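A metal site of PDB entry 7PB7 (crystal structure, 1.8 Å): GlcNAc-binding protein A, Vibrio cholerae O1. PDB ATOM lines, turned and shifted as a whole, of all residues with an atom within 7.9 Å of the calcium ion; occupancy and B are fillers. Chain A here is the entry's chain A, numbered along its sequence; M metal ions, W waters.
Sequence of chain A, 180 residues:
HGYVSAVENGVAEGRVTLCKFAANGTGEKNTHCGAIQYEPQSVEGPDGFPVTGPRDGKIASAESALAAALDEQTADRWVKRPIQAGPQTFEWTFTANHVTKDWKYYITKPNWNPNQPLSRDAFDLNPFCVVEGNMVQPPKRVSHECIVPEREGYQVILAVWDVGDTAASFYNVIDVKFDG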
ATOM      1  N   GLU A  44      -2.119  17.019 -20.401  1.00  0.00           N
ATOM      2  CA  GLU A  44      -0.978  17.134 -19.505  1.00  0.00           C
ATOM      3  C   GLU A  44       0.299  17.336 -20.314  1.00  0.00           C
ATOM      4  O   GLU A  44       0.503  16.666 -21.332  1.00  0.00           O
ATOM      5  CB  GLU A  44      -0.851  15.869 -18.632  1.00  0.00           C
ATOM      6  CG  GLU A  44       0.119  16.008 -17.461  1.00  0.00           C
ATOM      7  CD  GLU A  44       0.327  14.701 -16.707  1.00  0.00           C
ATOM      8  OE1 GLU A  44       0.084  13.623 -17.290  1.00  0.00           O
ATOM      9  OE2 GLU A  44       0.724  14.744 -15.529  1.00  0.00           O
ATOM     10  N   GLY A  45       1.134  18.278 -19.888  1.00  0.00           N
ATOM     11  CA  GLY A  45       2.351  18.596 -20.592  1.00  0.00           C
ATOM     12  C   GLY A  45       3.440  19.082 -19.659  1.00  0.00           C
ATOM     13  O   GLY A  45       3.216  19.242 -18.447  1.00  0.00           O
ATOM     14  N   PRO A  46       4.644  19.319 -20.188  1.00  0.00           N
ATOM     15  CA  PRO A  46       5.760  19.725 -19.328  1.00  0.00           C
ATOM     16  C   PRO A  46       5.562  21.084 -18.686  1.00  0.00           C
ATOM     17  O   PRO A  46       5.007  22.015 -19.279  1.00  0.00           O
ATOM     18  CB  PRO A  46       6.960  19.718 -20.279  1.00  0.00           C
ATOM     19  CG  PRO A  46       6.367  19.832 -21.646  1.00  0.00           C
ATOM     20  CD  PRO A  46       5.068  19.091 -21.577  1.00  0.00           C
ATOM     21  N   ASP A  47       6.049  21.191 -17.442  1.00  0.00           N
ATOM     22  CA  ASP A  47       6.101  22.446 -16.696  1.00  0.00           C
ATOM     23  C   ASP A  47       6.805  23.568 -17.438  1.00  0.00           C
ATOM     24  O   ASP A  47       7.672  23.317 -18.273  1.00  0.00           O
ATOM     25  CB  ASP A  47       6.849  22.239 -15.379  1.00  0.00           C
ATOM     26  CG  ASP A  47       6.017  21.565 -14.329  1.00  0.00           C
ATOM     27  OD1 ASP A  47       4.782  21.519 -14.483  1.00  0.00           O
ATOM     28  OD2 ASP A  47       6.611  21.084 -13.341  1.00  0.00           O
ATOM     29  N   GLY A  48       6.461  24.809 -17.087  1.00  0.00           N
ATOM     30  CA  GLY A  48       7.357  25.928 -17.272  1.00  0.00           C
ATOM     31  C   GLY A  48       7.045  26.863 -18.418  1.00  0.00           C
ATOM     32  O   GLY A  48       7.902  27.692 -18.748  1.00  0.00           O
ATOM     33  N   VAL A  99      -1.908  17.522  -5.642  1.00  0.00           N
ATOM     34  CA  VAL A  99      -1.208  18.614  -4.953  1.00  0.00           C
ATOM     35  C   VAL A  99      -0.826  19.668  -5.980  1.00  0.00           C
ATOM     36  O   VAL A  99      -0.305  19.351  -7.050  1.00  0.00           O
ATOM     37  CB  VAL A  99       0.025  18.056  -4.218  1.00  0.00           C
ATOM     38  CG1 VAL A  99       0.936  19.190  -3.750  1.00  0.00           C
ATOM     39  CG2 VAL A  99      -0.389  17.169  -3.044  1.00  0.00           C
ATOM     40  N   THR A 100      -1.086  20.934  -5.655  1.00  0.00           N
ATOM     41  CA  THR A 100      -1.030  22.012  -6.631  1.00  0.00           C
ATOM     42  C   THR A 100      -0.031  23.081  -6.233  1.00  0.00           C
ATOM     43  O   THR A 100      -0.030  23.542  -5.088  1.00  0.00           O
ATOM     44  CB  THR A 100      -2.419  22.626  -6.828  1.00  0.00           C
ATOM     45  OG1 THR A 100      -3.281  21.669  -7.436  1.00  0.00           O
ATOM     46  CG2 THR A 100      -2.334  23.854  -7.725  1.00  0.00           C
ATOM     47  N   LYS A 101       0.809  23.473  -7.187  1.00  0.00           N
ATOM     48  CA  LYS A 101       1.694  24.624  -6.989  1.00  0.00           C
ATOM     49  C   LYS A 101       0.930  25.933  -7.201  1.00  0.00           C
ATOM     50  O   LYS A 101       0.799  26.744  -6.273  1.00  0.00           O
ATOM     51  CB  LYS A 101       2.891  24.517  -7.946  1.00  0.00           C
ATOM     52  CG  LYS A 101       3.947  25.595  -7.746  1.00  0.00           C
ATOM     53  CD  LYS A 101       5.181  25.258  -8.583  1.00  0.00           C
ATOM     54  CE  LYS A 101       6.255  26.327  -8.453  1.00  0.00           C
ATOM     55  NZ  LYS A 101       7.489  25.959  -9.201  1.00  0.00           N
ATOM     56  N   ASP A 102       0.404  26.147  -8.400  1.00  0.00           N
ATOM     57  CA  ASP A 102      -0.428  27.321  -8.640  1.00  0.00           C
ATOM     58  C   ASP A 102      -1.224  27.129  -9.919  1.00  0.00           C
ATOM     59  O   ASP A 102      -1.073  26.132 -10.635  1.00  0.00           O
ATOM     60  CB  ASP A 102       0.414  28.614  -8.707  1.00  0.00           C
ATOM     61  CG  ASP A 102       1.590  28.512  -9.674  1.00  0.00           C
ATOM     62  OD1 ASP A 102       1.463  27.891 -10.752  1.00  0.00           O
ATOM     63  OD2 ASP A 102       2.656  29.101  -9.358  1.00  0.00           O
ATOM     64  N   TRP A 161      -2.542  24.819 -15.008  1.00  0.00           N
ATOM     65  CA  TRP A 161      -2.605  24.230 -13.677  1.00  0.00           C
ATOM     66  C   TRP A 161      -1.307  23.467 -13.440  1.00  0.00           C
ATOM     67  O   TRP A 161      -1.043  22.467 -14.102  1.00  0.00           O
ATOM     68  CB  TRP A 161      -3.828  23.310 -13.544  1.00  0.00           C
ATOM     69  CG  TRP A 161      -3.881  22.476 -12.285  1.00  0.00           C
ATOM     70  CD1 TRP A 161      -3.468  22.845 -11.030  1.00  0.00           C
ATOM     71  CD2 TRP A 161      -4.378  21.135 -12.158  1.00  0.00           C
ATOM     72  NE1 TRP A 161      -3.682  21.809 -10.137  1.00  0.00           N
ATOM     73  CE2 TRP A 161      -4.246  20.761 -10.810  1.00  0.00           C
ATOM     74  CE3 TRP A 161      -4.948  20.226 -13.074  1.00  0.00           C
ATOM     75  CZ2 TRP A 161      -4.630  19.497 -10.345  1.00  0.00           C
ATOM     76  CZ3 TRP A 161      -5.334  18.976 -12.609  1.00  0.00           C
ATOM     77  CH2 TRP A 161      -5.161  18.621 -11.258  1.00  0.00           C
ATOM     78  N   ASP A 162      -0.475  23.966 -12.536  1.00  0.00           N
ATOM     79  CA  ASP A 162       0.844  23.391 -12.299  1.00  0.00           C
ATOM     80  C   ASP A 162       0.740  22.413 -11.129  1.00  0.00           C
ATOM     81  O   ASP A 162       0.583  22.819  -9.972  1.00  0.00           O
ATOM     82  CB  ASP A 162       1.888  24.486 -12.029  1.00  0.00           C
ATOM     83  CG  ASP A 162       3.310  23.946 -11.978  1.00  0.00           C
ATOM     84  OD1 ASP A 162       3.478  22.706 -11.873  1.00  0.00           O
ATOM     85  OD2 ASP A 162       4.266  24.754 -12.055  1.00  0.00           O
ATOM     86  N   VAL A 163       0.803  21.124 -11.452  1.00  0.00           N
ATOM     87  CA  VAL A 163       0.791  20.085 -10.432  1.00  0.00           C
ATOM     88  C   VAL A 163       2.099  20.154  -9.663  1.00  0.00           C
ATOM     89  O   VAL A 163       3.187  20.132 -10.258  1.00  0.00           O
ATOM     90  CB  VAL A 163       0.570  18.712 -11.069  1.00  0.00           C
ATOM     91  CG1 VAL A 163       0.743  17.602 -10.037  1.00  0.00           C
ATOM     92  CG2 VAL A 163      -0.816  18.656 -11.710  1.00  0.00           C
ATOM     93  N   GLY A 164       2.007  20.239  -8.330  1.00  0.00           N
ATOM     94  CA  GLY A 164       3.170  20.560  -7.513  1.00  0.00           C
ATOM     95  C   GLY A 164       4.117  19.417  -7.197  1.00  0.00           C
ATOM     96  O   GLY A 164       5.253  19.675  -6.785  1.00  0.00           O
ATOM     97  N   ASP A 165       3.685  18.161  -7.354  1.00  0.00           N
ATOM     98  CA  ASP A 165       4.565  17.046  -7.040  1.00  0.00           C
ATOM     99  C   ASP A 165       5.023  16.280  -8.264  1.00  0.00           C
ATOM    100  O   ASP A 165       5.573  15.184  -8.130  1.00  0.00           O
ATOM    101  CB  ASP A 165       3.908  16.096  -6.027  1.00  0.00           C
ATOM    102  CG  ASP A 165       2.521  15.665  -6.436  1.00  0.00           C
ATOM    103  OD1 ASP A 165       2.025  16.126  -7.492  1.00  0.00           O
ATOM    104  OD2 ASP A 165       1.906  14.881  -5.685  1.00  0.00           O
ATOM    105  N   THR A 166       4.808  16.823  -9.467  1.00  0.00           N
ATOM    106  CA  THR A 166       5.356  16.267 -10.698  1.00  0.00           C
ATOM    107  C   THR A 166       5.928  17.400 -11.544  1.00  0.00           C
ATOM    108  O   THR A 166       5.639  18.581 -11.315  1.00  0.00           O
ATOM    109  CB  THR A 166       4.309  15.511 -11.523  1.00  0.00           C
ATOM    110  OG1 THR A 166       3.491  16.465 -12.214  1.00  0.00           O
ATOM    111  CG2 THR A 166       3.437  14.627 -10.655  1.00  0.00           C
ATOM    112  N   ALA A 167       6.743  17.035 -12.526  1.00  0.00           N
ATOM    113  CA  ALA A 167       7.268  17.996 -13.482  1.00  0.00           C
ATOM    114  C   ALA A 167       6.272  18.356 -14.580  1.00  0.00           C
ATOM    115  O   ALA A 167       6.692  18.847 -15.644  1.00  0.00           O
ATOM    116  CB  ALA A 167       8.552  17.465 -14.127  1.00  0.00           C
ATOM    117  N   ALA A 168       4.974  18.164 -14.353  1.00  0.00           N
ATOM    118  CA  ALA A 168       3.953  18.347 -15.371  1.00  0.00           C
ATOM    119  C   ALA A 168       2.943  19.420 -14.961  1.00  0.00           C
ATOM    120  O   ALA A 168       2.762  19.715 -13.780  1.00  0.00           O
ATOM    121  CB  ALA A 168       3.204  17.046 -15.661  1.00  0.00           C
ATOM    122  N   SER A 169       2.311  19.998 -15.975  1.00  0.00           N
ATOM    123  CA  SER A 169       1.211  20.944 -15.815  1.00  0.00           C
ATOM    124  C   SER A 169       0.112  20.559 -16.783  1.00  0.00           C
ATOM    125  O   SER A 169       0.334  19.832 -17.753  1.00  0.00           O
ATOM    126  CB  SER A 169       1.660  22.386 -16.099  1.00  0.00           C
ATOM    127  OG  SER A 169       2.532  22.869 -15.073  1.00  0.00           O
ATOM    128  N   PHE A 170      -1.091  21.068 -16.528  1.00  0.00           N
ATOM    129  CA  PHE A 170      -2.225  20.897 -17.426  1.00  0.00           C
ATOM    130  C   PHE A 170      -2.537  22.217 -18.093  1.00  0.00           C
ATOM    131  O   PHE A 170      -2.612  23.246 -17.423  1.00  0.00           O
ATOM    132  CB  PHE A 170      -3.438  20.356 -16.683  1.00  0.00           C
ATOM    133  CG  PHE A 170      -3.301  18.914 -16.279  1.00  0.00           C
ATOM    134  CD1 PHE A 170      -2.549  18.567 -15.169  1.00  0.00           C
ATOM    135  CD2 PHE A 170      -3.858  17.907 -17.040  1.00  0.00           C
ATOM    136  CE1 PHE A 170      -2.388  17.236 -14.799  1.00  0.00           C
ATOM    137  CE2 PHE A 170      -3.710  16.575 -16.691  1.00  0.00           C
ATOM    138  CZ  PHE A 170      -2.969  16.248 -15.560  1.00  0.00           C
HETATM  139 CA    CA M   1       4.498  20.563 -12.086  1.00  0.00          CA
HETATM  140  O   HOH W   1       6.113  21.498 -10.442  1.00  0.00           O
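The backbone NH (N) of Ala 168 lies close to the side-chain hydroxyl (OG1) of Thr 166, at 3.1 Å.
N of Asp 162 is in hydrogen-bond range of O of Asp 102 (2.9 Å).
OD1 of Asp 162 lies close to OG of Ser 169, at 3.3 Å.
N of Lys 101 sits at hydrogen-bond distance from O of Asp 162.
N of Asp 47 lies within hydrogen-bond range of O of Ala 167, at 3.0 Å.
The side-chain carboxylate (OD1) of Asp 47 lies close to the side-chain hydroxyl (OG) of Ser 169 (2.7 Å).
The calcium ion is bound by the backbone carbonyl oxygen (O) of Val 163 (2.3 Å), the side-chain carboxylate (OD1) of Asp 162 (2.4 Å), the backbone carbonyl oxygen (O) of Thr 166 (2.4 Å), water W1 (2.5 Å), the side-chain carboxylate (OD2) of Asp 47 (2.5 Å), the backbone carbonyl oxygen (O) of Ala 168 (2.6 Å) and the side-chain carboxylate (OD1) of Asp 47 (2.6 Å).
Residues that only touch the calcium ion: Ala 167 (3.8 Å).
Within 4 Å of the calcium ion: Asp 47, Asp 162, Val 163, Thr 166, Ala 167 and Ala 168.
The nearest printed residue that does not touch the calcium ion is Ser 169 (4.3 Å).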
